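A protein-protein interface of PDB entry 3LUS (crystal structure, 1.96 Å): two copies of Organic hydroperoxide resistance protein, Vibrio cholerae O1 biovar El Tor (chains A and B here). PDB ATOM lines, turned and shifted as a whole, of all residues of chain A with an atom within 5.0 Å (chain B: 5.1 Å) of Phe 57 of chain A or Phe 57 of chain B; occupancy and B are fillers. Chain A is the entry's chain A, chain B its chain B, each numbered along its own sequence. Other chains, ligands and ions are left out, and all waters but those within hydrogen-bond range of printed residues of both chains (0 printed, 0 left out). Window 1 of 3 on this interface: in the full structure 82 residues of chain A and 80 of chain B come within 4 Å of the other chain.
Among the printed residues, pairs that only touch across the chains: Tyr 129 of chain A with Phe 57 of chain B (3.5 Å), Phe 57 of chain A with Tyr 129 of chain B (3.5 Å), Gly 60 of chain A with Pro 53 of chain B (3.7 Å), Leu 56 of chain A with Val 59 of chain B (3.7 Å), Val 59 of chain A with Leu 56 of chain B (3.7 Å), Leu 56 of chain A with Leu 56 of chain B (3.7 Å), Pro 53 of chain A with Gly 60 of chain B (3.8 Å), Gly 60 of chain A with Leu 56 of chain B (3.8 Å) and Phe 57 of chain A with Phe 57 of chain B (3.9 Å).
Hydrophobic or aromatic side chains of chain B within 4 Å of the printed part of chain A: Pro 53, Leu 56, Phe 57, Val 59 and Tyr 129.
Along chain B the printed residues that touch a printed residue of chain A span positions 53 to 129.
Of the 16 printed residues of chain A, 6 touch a printed residue of chain B.
Hydrophobic or aromatic side chains of chain A that line the printed part of chain B: Pro 53, Leu 56, Phe 57, Val 59 and Tyr 129.
Among the printed residues, no Asp or Glu carboxylate lies within 4 Å of a Lys or Arg side-chain nitrogen of the other chain.
Pro 53 of chain A touches Tyr 129 of chain B, and with the chains exchanged Tyr 129 of chain A touches Pro 53 of chain B.
Leu 56 of chain A touches its own counterpart, Leu 56 of chain B.
Phe 57 of chain B touches its own counterpart, Phe 57 of chain A.
Gly 60 of chain A touches Leu 56 of chain B, but with the chains exchanged Leu 56 of chain A does not touch Gly 60 of chain B (4.01 Å).
Positions printed for both chains: 53, 54, 55, 56, 57, 58, 59, 60, 61, 62, 89, 101, 103, 129, 133 and 137.
Of the 11 pairs that touch across the chains among the printed residues, 10 have their exchanged pair printed and touching as well.
OH of Tyr 129 of chain B sits at hydrogen-bond distance from O of Pro 53 of chain A, 2.7 Å away.
O of Pro 53 of chain B lies within hydrogen-bond range of OH of Tyr 129 of chain A, 2.7 Å away.
Of chain B, only Phe 57 (3.9 Å) and Tyr 129 (3.5 Å) come within 4 Å of Phe 57 of chain A.
Of the printed residues of chain A, Phe 57 of chain B touches Phe 57 (3.9 Å) and Tyr 129 (3.5 Å).
Printed residues of chain A within 4 Å of Tyr 129 of chain B: Pro 53 and Phe 57.
Of the printed residues of chain A, Pro 53 of chain B touches Gly 60 (3.7 Å) and Tyr 129 (2.7 Å).
Ala 58 of chain B touches none of the printed residues of chain A.
Ala 62 of chain A touches none of the printed residues of chain B.
The nearest printed residue of chain B that does not touch Phe 57 of chain A is Leu 56 of chain B (5.7 Å).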
ATOM      1  N   PRO A  53      -1.997 -33.243  22.098  1.00  0.00           N
ATOM      2  CA  PRO A  53      -2.103 -32.257  21.003  1.00  0.00           C
ATOM      3  C   PRO A  53      -3.520 -31.858  20.717  1.00  0.00           C
ATOM      4  O   PRO A  53      -3.742 -30.737  20.313  1.00  0.00           O
ATOM      5  CB  PRO A  53      -1.523 -32.994  19.820  1.00  0.00           C
ATOM      6  CG  PRO A  53      -0.568 -33.955  20.456  1.00  0.00           C
ATOM      7  CD  PRO A  53      -1.229 -34.431  21.680  1.00  0.00           C
ATOM      8  N   GLU A  54      -4.502 -32.733  20.933  1.00  0.00           N
ATOM      9  CA  GLU A  54      -5.915 -32.357  20.705  1.00  0.00           C
ATOM     10  C   GLU A  54      -6.433 -31.328  21.696  1.00  0.00           C
ATOM     11  O   GLU A  54      -7.153 -30.366  21.306  1.00  0.00           O
ATOM     12  CB  GLU A  54      -6.851 -33.578  20.622  1.00  0.00           C
ATOM     13  CG  GLU A  54      -6.686 -34.298  19.276  1.00  0.00           C
ATOM     14  CD  GLU A  54      -5.324 -34.969  19.204  1.00  0.00           C
ATOM     15  OE1 GLU A  54      -4.973 -35.627  20.198  1.00  0.00           O
ATOM     16  OE2 GLU A  54      -4.580 -34.805  18.203  1.00  0.00           O
ATOM     17  N   GLN A  55      -6.077 -31.471  22.975  1.00  0.00           N
ATOM     18  CA  GLN A  55      -6.413 -30.473  23.965  1.00  0.00           C
ATOM     19  C   GLN A  55      -5.699 -29.180  23.696  1.00  0.00           C
ATOM     20  O   GLN A  55      -6.209 -28.087  23.942  1.00  0.00           O
ATOM     21  CB  GLN A  55      -5.958 -30.925  25.396  1.00  0.00           C
ATOM     22  CG  GLN A  55      -6.908 -31.736  26.023  1.00  0.00           C
ATOM     23  CD  GLN A  55      -6.732 -31.835  27.536  1.00  0.00           C
ATOM     24  OE1 GLN A  55      -5.666 -31.572  28.090  1.00  0.00           O
ATOM     25  NE2 GLN A  55      -7.776 -32.241  28.172  1.00  0.00           N
ATOM     26  N   LEU A  56      -4.442 -29.284  23.284  1.00  0.00           N
ATOM     27  CA  LEU A  56      -3.682 -28.055  22.941  1.00  0.00           C
ATOM     28  C   LEU A  56      -4.353 -27.286  21.819  1.00  0.00           C
ATOM     29  O   LEU A  56      -4.367 -26.032  21.788  1.00  0.00           O
ATOM     30  CB  LEU A  56      -2.239 -28.361  22.559  1.00  0.00           C
ATOM     31  CG  LEU A  56      -1.396 -28.715  23.798  1.00  0.00           C
ATOM     32  CD1 LEU A  56      -0.134 -29.542  23.508  1.00  0.00           C
ATOM     33  CD2 LEU A  56      -0.997 -27.439  24.518  1.00  0.00           C
ATOM     34  N   PHE A  57      -4.877 -28.024  20.867  1.00  0.00           N
ATOM     35  CA  PHE A  57      -5.509 -27.339  19.736  1.00  0.00           C
ATOM     36  C   PHE A  57      -6.811 -26.688  20.225  1.00  0.00           C
ATOM     37  O   PHE A  57      -7.137 -25.560  19.861  1.00  0.00           O
ATOM     38  CB  PHE A  57      -5.795 -28.339  18.645  1.00  0.00           C
ATOM     39  CG  PHE A  57      -6.237 -27.704  17.371  1.00  0.00           C
ATOM     40  CD1 PHE A  57      -5.364 -26.901  16.655  1.00  0.00           C
ATOM     41  CD2 PHE A  57      -7.520 -27.845  16.924  1.00  0.00           C
ATOM     42  CE1 PHE A  57      -5.767 -26.304  15.483  1.00  0.00           C
ATOM     43  CE2 PHE A  57      -7.913 -27.270  15.761  1.00  0.00           C
ATOM     44  CZ  PHE A  57      -7.050 -26.508  15.033  1.00  0.00           C
ATOM     45  N   ALA A  58      -7.558 -27.383  21.084  1.00  0.00           N
ATOM     46  CA  ALA A  58      -8.801 -26.818  21.661  1.00  0.00           C
ATOM     47  C   ALA A  58      -8.550 -25.516  22.465  1.00  0.00           C
ATOM     48  O   ALA A  58      -9.287 -24.516  22.364  1.00  0.00           O
ATOM     49  CB  ALA A  58      -9.572 -27.896  22.526  1.00  0.00           C
ATOM     50  N   VAL A  59      -7.499 -25.544  23.260  1.00  0.00           N
ATOM     51  CA  VAL A  59      -7.129 -24.433  24.095  1.00  0.00           C
ATOM     52  C   VAL A  59      -6.677 -23.295  23.229  1.00  0.00           C
ATOM     53  O   VAL A  59      -7.138 -22.140  23.345  1.00  0.00           O
ATOM     54  CB  VAL A  59      -6.003 -24.887  25.053  1.00  0.00           C
ATOM     55  CG1 VAL A  59      -5.229 -23.727  25.543  1.00  0.00           C
ATOM     56  CG2 VAL A  59      -6.618 -25.790  26.229  1.00  0.00           C
ATOM     57  N   GLY A  60      -5.820 -23.593  22.276  1.00  0.00           N
ATOM     58  CA  GLY A  60      -5.332 -22.544  21.419  1.00  0.00           C
ATOM     59  C   GLY A  60      -6.384 -21.962  20.523  1.00  0.00           C
ATOM     60  O   GLY A  60      -6.399 -20.735  20.315  1.00  0.00           O
ATOM     61  N   TYR A  61      -7.240 -22.801  19.961  1.00  0.00           N
ATOM     62  CA  TYR A  61      -8.358 -22.324  19.086  1.00  0.00           C
ATOM     63  C   TYR A  61      -9.383 -21.511  19.895  1.00  0.00           C
ATOM     64  O   TYR A  61      -9.785 -20.411  19.487  1.00  0.00           O
ATOM     65  CB  TYR A  61      -9.027 -23.467  18.353  1.00  0.00           C
ATOM     66  CG  TYR A  61      -9.712 -23.070  17.038  1.00  0.00           C
ATOM     67  CD1 TYR A  61     -10.006 -24.024  16.074  1.00  0.00           C
ATOM     68  CD2 TYR A  61      -9.948 -21.737  16.704  1.00  0.00           C
ATOM     69  CE1 TYR A  61     -10.585 -23.689  14.894  1.00  0.00           C
ATOM     70  CE2 TYR A  61     -10.589 -21.401  15.481  1.00  0.00           C
ATOM     71  CZ  TYR A  61     -10.928 -22.381  14.622  1.00  0.00           C
ATOM     72  OH  TYR A  61     -11.515 -22.030  13.421  1.00  0.00           O
ATOM     73  N   ALA A  62      -9.741 -21.972  21.094  1.00  0.00           N
ATOM     74  CA  ALA A  62     -10.654 -21.165  21.938  1.00  0.00           C
ATOM     75  C   ALA A  62     -10.045 -19.809  22.191  1.00  0.00           C
ATOM     76  O   ALA A  62     -10.714 -18.804  22.064  1.00  0.00           O
ATOM     77  CB  ALA A  62     -11.032 -21.874  23.278  1.00  0.00           C
ATOM     78  N   VAL A  89     -12.917 -30.272  20.396  1.00  0.00           N
ATOM     79  CA  VAL A  89     -12.116 -30.846  19.371  1.00  0.00           C
ATOM     80  C   VAL A  89     -12.194 -32.385  19.464  1.00  0.00           C
ATOM     81  O   VAL A  89     -12.000 -32.966  20.522  1.00  0.00           O
ATOM     82  CB  VAL A  89     -10.631 -30.343  19.424  1.00  0.00           C
ATOM     83  CG1 VAL A  89      -9.718 -31.158  18.398  1.00  0.00           C
ATOM     84  CG2 VAL A  89     -10.494 -28.752  19.202  1.00  0.00           C
ATOM     85  N   LEU A 101      -9.174 -33.938  12.478  1.00  0.00           N
ATOM     86  CA  LEU A 101      -9.789 -33.207  13.559  1.00  0.00           C
ATOM     87  C   LEU A 101     -11.132 -32.698  13.124  1.00  0.00           C
ATOM     88  O   LEU A 101     -11.324 -32.259  11.988  1.00  0.00           O
ATOM     89  CB  LEU A 101      -8.913 -32.012  14.005  1.00  0.00           C
ATOM     90  CG  LEU A 101      -7.506 -32.308  14.464  1.00  0.00           C
ATOM     91  CD1 LEU A 101      -6.814 -30.997  14.879  1.00  0.00           C
ATOM     92  CD2 LEU A 101      -7.507 -33.361  15.555  1.00  0.00           C
ATOM     93  N   VAL A 103     -13.997 -29.871  14.813  1.00  0.00           N
ATOM     94  CA  VAL A 103     -14.041 -28.706  15.694  1.00  0.00           C
ATOM     95  C   VAL A 103     -15.410 -27.989  15.763  1.00  0.00           C
ATOM     96  O   VAL A 103     -16.053 -27.679  14.728  1.00  0.00           O
ATOM     97  CB  VAL A 103     -13.003 -27.609  15.261  1.00  0.00           C
ATOM     98  CG1 VAL A 103     -13.023 -26.458  16.346  1.00  0.00           C
ATOM     99  CG2 VAL A 103     -11.591 -28.250  15.137  1.00  0.00           C
ATOM    100  N   TYR A 129      -6.328 -19.285  13.185  1.00  0.00           N
ATOM    101  CA  TYR A 129      -6.685 -20.703  13.229  1.00  0.00           C
ATOM    102  C   TYR A 129      -7.795 -21.014  12.199  1.00  0.00           C
ATOM    103  O   TYR A 129      -7.750 -22.076  11.516  1.00  0.00           O
ATOM    104  CB  TYR A 129      -7.166 -21.136  14.598  1.00  0.00           C
ATOM    105  CG  TYR A 129      -6.083 -21.519  15.635  1.00  0.00           C
ATOM    106  CD1 TYR A 129      -6.187 -22.693  16.357  1.00  0.00           C
ATOM    107  CD2 TYR A 129      -5.019 -20.685  15.916  1.00  0.00           C
ATOM    108  CE1 TYR A 129      -5.252 -23.037  17.348  1.00  0.00           C
ATOM    109  CE2 TYR A 129      -4.101 -21.003  16.924  1.00  0.00           C
ATOM    110  CZ  TYR A 129      -4.219 -22.186  17.618  1.00  0.00           C
ATOM    111  OH  TYR A 129      -3.316 -22.545  18.603  1.00  0.00           O
ATOM    112  N   VAL A 133      -7.457 -23.726   8.863  1.00  0.00           N
ATOM    113  CA  VAL A 133      -8.199 -24.948   8.648  1.00  0.00           C
ATOM    114  C   VAL A 133      -9.379 -24.828   7.642  1.00  0.00           C
ATOM    115  O   VAL A 133     -10.066 -25.815   7.376  1.00  0.00           O
ATOM    116  CB  VAL A 133      -8.753 -25.481   9.974  1.00  0.00           C
ATOM    117  CG1 VAL A 133      -7.579 -25.607  11.013  1.00  0.00           C
ATOM    118  CG2 VAL A 133      -9.865 -24.646  10.486  1.00  0.00           C
ATOM    119  N   ILE A 137     -11.403 -28.490   7.778  1.00  0.00           N
ATOM    120  CA  ILE A 137     -12.333 -28.726   8.837  1.00  0.00           C
ATOM    121  C   ILE A 137     -13.560 -27.835   8.656  1.00  0.00           C
ATOM    122  O   ILE A 137     -13.431 -26.596   8.496  1.00  0.00           O
ATOM    123  CB  ILE A 137     -11.635 -28.399  10.195  1.00  0.00           C
ATOM    124  CG1 ILE A 137     -10.383 -29.226  10.336  1.00  0.00           C
ATOM    125  CG2 ILE A 137     -12.613 -28.701  11.296  1.00  0.00           C
ATOM    126  CD1 ILE A 137      -9.541 -28.854  11.606  1.00  0.00           C
ATOM    127  N   PRO B  53      -1.878 -18.148  21.420  1.00  0.00           N
ATOM    128  CA  PRO B  53      -2.289 -19.225  20.520  1.00  0.00           C
ATOM    129  C   PRO B  53      -1.220 -19.724  19.562  1.00  0.00           C
ATOM    130  O   PRO B  53      -1.267 -20.870  19.154  1.00  0.00           O
ATOM    131  CB  PRO B  53      -3.464 -18.622  19.770  1.00  0.00           C
ATOM    132  CG  PRO B  53      -3.976 -17.572  20.693  1.00  0.00           C
ATOM    133  CD  PRO B  53      -2.788 -16.986  21.307  1.00  0.00           C
ATOM    134  N   GLU B  54      -0.206 -18.922  19.278  1.00  0.00           N
ATOM    135  CA  GLU B  54       0.876 -19.388  18.403  1.00  0.00           C
ATOM    136  C   GLU B  54       1.824 -20.351  19.126  1.00  0.00           C
ATOM    137  O   GLU B  54       2.272 -21.390  18.564  1.00  0.00           O
ATOM    138  CB  GLU B  54       1.648 -18.205  17.847  1.00  0.00           C
ATOM    139  CG  GLU B  54       0.867 -17.459  16.800  1.00  0.00           C
ATOM    140  CD  GLU B  54      -0.316 -16.647  17.343  1.00  0.00           C
ATOM    141  OE1 GLU B  54      -0.235 -16.094  18.472  1.00  0.00           O
ATOM    142  OE2 GLU B  54      -1.333 -16.582  16.624  1.00  0.00           O
ATOM    143  N   GLN B  55       2.113 -20.034  20.383  1.00  0.00           N
ATOM    144  CA  GLN B  55       2.892 -20.940  21.146  1.00  0.00           C
ATOM    145  C   GLN B  55       2.178 -22.244  21.309  1.00  0.00           C
ATOM    146  O   GLN B  55       2.820 -23.263  21.232  1.00  0.00           O
ATOM    147  CB  GLN B  55       3.282 -20.392  22.529  1.00  0.00           C
ATOM    148  CG  GLN B  55       4.166 -19.197  22.497  1.00  0.00           C
ATOM    149  CD  GLN B  55       4.641 -18.820  23.887  1.00  0.00           C
ATOM    150  OE1 GLN B  55       4.021 -19.182  24.904  1.00  0.00           O
ATOM    151  NE2 GLN B  55       5.704 -18.045  23.933  1.00  0.00           N
ATOM    152  N   LEU B  56       0.886 -22.222  21.610  1.00  0.00           N
ATOM    153  CA  LEU B  56       0.143 -23.441  21.811  1.00  0.00           C
ATOM    154  C   LEU B  56       0.100 -24.298  20.521  1.00  0.00           C
ATOM    155  O   LEU B  56       0.218 -25.528  20.554  1.00  0.00           O
ATOM    156  CB  LEU B  56      -1.271 -23.087  22.289  1.00  0.00           C
ATOM    157  CG  LEU B  56      -1.334 -22.556  23.735  1.00  0.00           C
ATOM    158  CD1 LEU B  56      -2.572 -21.708  23.911  1.00  0.00           C
ATOM    159  CD2 LEU B  56      -1.314 -23.710  24.710  1.00  0.00           C
ATOM    160  N   PHE B  57      -0.058 -23.624  19.396  1.00  0.00           N
ATOM    161  CA  PHE B  57      -0.033 -24.283  18.083  1.00  0.00           C
ATOM    162  C   PHE B  57       1.322 -24.924  17.792  1.00  0.00           C
ATOM    163  O   PHE B  57       1.368 -26.085  17.359  1.00  0.00           O
ATOM    164  CB  PHE B  57      -0.384 -23.326  16.949  1.00  0.00           C
ATOM    165  CG  PHE B  57      -0.670 -24.019  15.682  1.00  0.00           C
ATOM    166  CD1 PHE B  57      -1.754 -24.911  15.615  1.00  0.00           C
ATOM    167  CD2 PHE B  57       0.085 -23.800  14.542  1.00  0.00           C
ATOM    168  CE1 PHE B  57      -2.078 -25.589  14.452  1.00  0.00           C
ATOM    169  CE2 PHE B  57      -0.257 -24.491  13.322  1.00  0.00           C
ATOM    170  CZ  PHE B  57      -1.297 -25.387  13.291  1.00  0.00           C
ATOM    171  N   ALA B  58       2.395 -24.204  18.129  1.00  0.00           N
ATOM    172  CA  ALA B  58       3.748 -24.735  17.966  1.00  0.00           C
ATOM    173  C   ALA B  58       3.982 -25.973  18.839  1.00  0.00           C
ATOM    174  O   ALA B  58       4.525 -26.945  18.364  1.00  0.00           O
ATOM    175  CB  ALA B  58       4.830 -23.655  18.250  1.00  0.00           C
ATOM    176  N   VAL B  59       3.600 -25.937  20.109  1.00  0.00           N
ATOM    177  CA  VAL B  59       3.806 -27.100  20.988  1.00  0.00           C
ATOM    178  C   VAL B  59       2.952 -28.249  20.487  1.00  0.00           C
ATOM    179  O   VAL B  59       3.408 -29.395  20.423  1.00  0.00           O
ATOM    180  CB  VAL B  59       3.425 -26.690  22.433  1.00  0.00           C
ATOM    181  CG1 VAL B  59       3.133 -27.850  23.340  1.00  0.00           C
ATOM    182  CG2 VAL B  59       4.530 -25.898  23.027  1.00  0.00           C
ATOM    183  N   GLY B  60       1.704 -27.975  20.091  1.00  0.00           N
ATOM    184  CA  GLY B  60       0.870 -29.036  19.658  1.00  0.00           C
ATOM    185  C   GLY B  60       1.317 -29.745  18.354  1.00  0.00           C
ATOM    186  O   GLY B  60       1.253 -30.970  18.241  1.00  0.00           O
ATOM    187  N   TYR B  61       1.688 -28.939  17.371  1.00  0.00           N
ATOM    188  CA  TYR B  61       2.147 -29.427  16.074  1.00  0.00           C
ATOM    189  C   TYR B  61       3.503 -30.122  16.209  1.00  0.00           C
ATOM    190  O   TYR B  61       3.728 -31.226  15.710  1.00  0.00           O
ATOM    191  CB  TYR B  61       2.269 -28.301  15.137  1.00  0.00           C
ATOM    192  CG  TYR B  61       2.049 -28.698  13.682  1.00  0.00           C
ATOM    193  CD1 TYR B  61       1.784 -27.733  12.726  1.00  0.00           C
ATOM    194  CD2 TYR B  61       2.095 -30.007  13.269  1.00  0.00           C
ATOM    195  CE1 TYR B  61       1.612 -28.084  11.384  1.00  0.00           C
ATOM    196  CE2 TYR B  61       1.941 -30.344  11.888  1.00  0.00           C
ATOM    197  CZ  TYR B  61       1.670 -29.398  10.999  1.00  0.00           C
ATOM    198  OH  TYR B  61       1.496 -29.751   9.661  1.00  0.00           O
ATOM    199  N   ALA B  62       4.398 -29.548  16.970  1.00  0.00           N
ATOM    200  CA  ALA B  62       5.654 -30.268  17.231  1.00  0.00           C
ATOM    201  C   ALA B  62       5.420 -31.669  17.852  1.00  0.00           C
ATOM    202  O   ALA B  62       6.057 -32.667  17.422  1.00  0.00           O
ATOM    203  CB  ALA B  62       6.584 -29.420  18.125  1.00  0.00           C
ATOM    204  N   VAL B  89       6.378 -21.275  14.306  1.00  0.00           N
ATOM    205  CA  VAL B  89       5.128 -20.695  13.890  1.00  0.00           C
ATOM    206  C   VAL B  89       5.221 -19.164  13.930  1.00  0.00           C
ATOM    207  O   VAL B  89       5.536 -18.566  14.973  1.00  0.00           O
ATOM    208  CB  VAL B  89       4.012 -21.130  14.829  1.00  0.00           C
ATOM    209  CG1 VAL B  89       2.611 -20.496  14.410  1.00  0.00           C
ATOM    210  CG2 VAL B  89       3.903 -22.666  14.878  1.00  0.00           C
ATOM    211  N   LEU B 101      -1.169 -17.886   9.673  1.00  0.00           N
ATOM    212  CA  LEU B 101      -0.017 -18.488  10.288  1.00  0.00           C
ATOM    213  C   LEU B 101       0.919 -18.946   9.189  1.00  0.00           C
ATOM    214  O   LEU B 101       0.505 -19.372   8.116  1.00  0.00           O
ATOM    215  CB  LEU B 101      -0.443 -19.712  11.113  1.00  0.00           C
ATOM    216  CG  LEU B 101      -1.374 -19.454  12.305  1.00  0.00           C
ATOM    217  CD1 LEU B 101      -1.794 -20.773  13.002  1.00  0.00           C
ATOM    218  CD2 LEU B 101      -0.829 -18.373  13.286  1.00  0.00           C
ATOM    219  N   VAL B 103       4.261 -21.806   9.066  1.00  0.00           N
ATOM    220  CA  VAL B 103       4.771 -22.925   9.914  1.00  0.00           C
ATOM    221  C   VAL B 103       5.908 -23.618   9.226  1.00  0.00           C
ATOM    222  O   VAL B 103       5.822 -23.925   8.017  1.00  0.00           O
ATOM    223  CB  VAL B 103       3.660 -23.994  10.214  1.00  0.00           C
ATOM    224  CG1 VAL B 103       4.188 -25.156  11.055  1.00  0.00           C
ATOM    225  CG2 VAL B 103       2.451 -23.364  10.947  1.00  0.00           C
ATOM    226  N   TYR B 129      -2.792 -32.586  12.439  1.00  0.00           N
ATOM    227  CA  TYR B 129      -2.524 -31.161  12.244  1.00  0.00           C
ATOM    228  C   TYR B 129      -2.182 -30.822  10.811  1.00  0.00           C
ATOM    229  O   TYR B 129      -2.652 -29.777  10.296  1.00  0.00           O
ATOM    230  CB  TYR B 129      -1.375 -30.694  13.129  1.00  0.00           C
ATOM    231  CG  TYR B 129      -1.727 -30.284  14.545  1.00  0.00           C
ATOM    232  CD1 TYR B 129      -1.313 -29.039  15.056  1.00  0.00           C
ATOM    233  CD2 TYR B 129      -2.347 -31.183  15.418  1.00  0.00           C
ATOM    234  CE1 TYR B 129      -1.548 -28.656  16.445  1.00  0.00           C
ATOM    235  CE2 TYR B 129      -2.609 -30.819  16.780  1.00  0.00           C
ATOM    236  CZ  TYR B 129      -2.176 -29.549  17.288  1.00  0.00           C
ATOM    237  OH  TYR B 129      -2.433 -29.181  18.593  1.00  0.00           O
ATOM    238  N   VAL B 133      -4.356 -28.325   8.113  1.00  0.00           N
ATOM    239  CA  VAL B 133      -3.897 -27.087   7.495  1.00  0.00           C
ATOM    240  C   VAL B 133      -3.532 -27.207   5.982  1.00  0.00           C
ATOM    241  O   VAL B 133      -3.134 -26.226   5.327  1.00  0.00           O
ATOM    242  CB  VAL B 133      -2.799 -26.425   8.328  1.00  0.00           C
ATOM    243  CG1 VAL B 133      -3.243 -26.282   9.805  1.00  0.00           C
ATOM    244  CG2 VAL B 133      -1.434 -27.207   8.243  1.00  0.00           C
ATOM    245  N   ILE B 137      -1.826 -23.562   4.768  1.00  0.00           N
ATOM    246  CA  ILE B 137      -0.510 -23.174   5.210  1.00  0.00           C
ATOM    247  C   ILE B 137       0.470 -24.017   4.370  1.00  0.00           C
ATOM    248  O   ILE B 137       0.310 -25.233   4.219  1.00  0.00           O
ATOM    249  CB  ILE B 137      -0.293 -23.467   6.723  1.00  0.00           C
ATOM    250  CG1 ILE B 137      -1.252 -22.675   7.609  1.00  0.00           C
ATOM    251  CG2 ILE B 137       1.182 -23.146   7.115  1.00  0.00           C
ATOM    252  CD1 ILE B 137      -1.129 -23.065   9.166  1.00  0.00           C
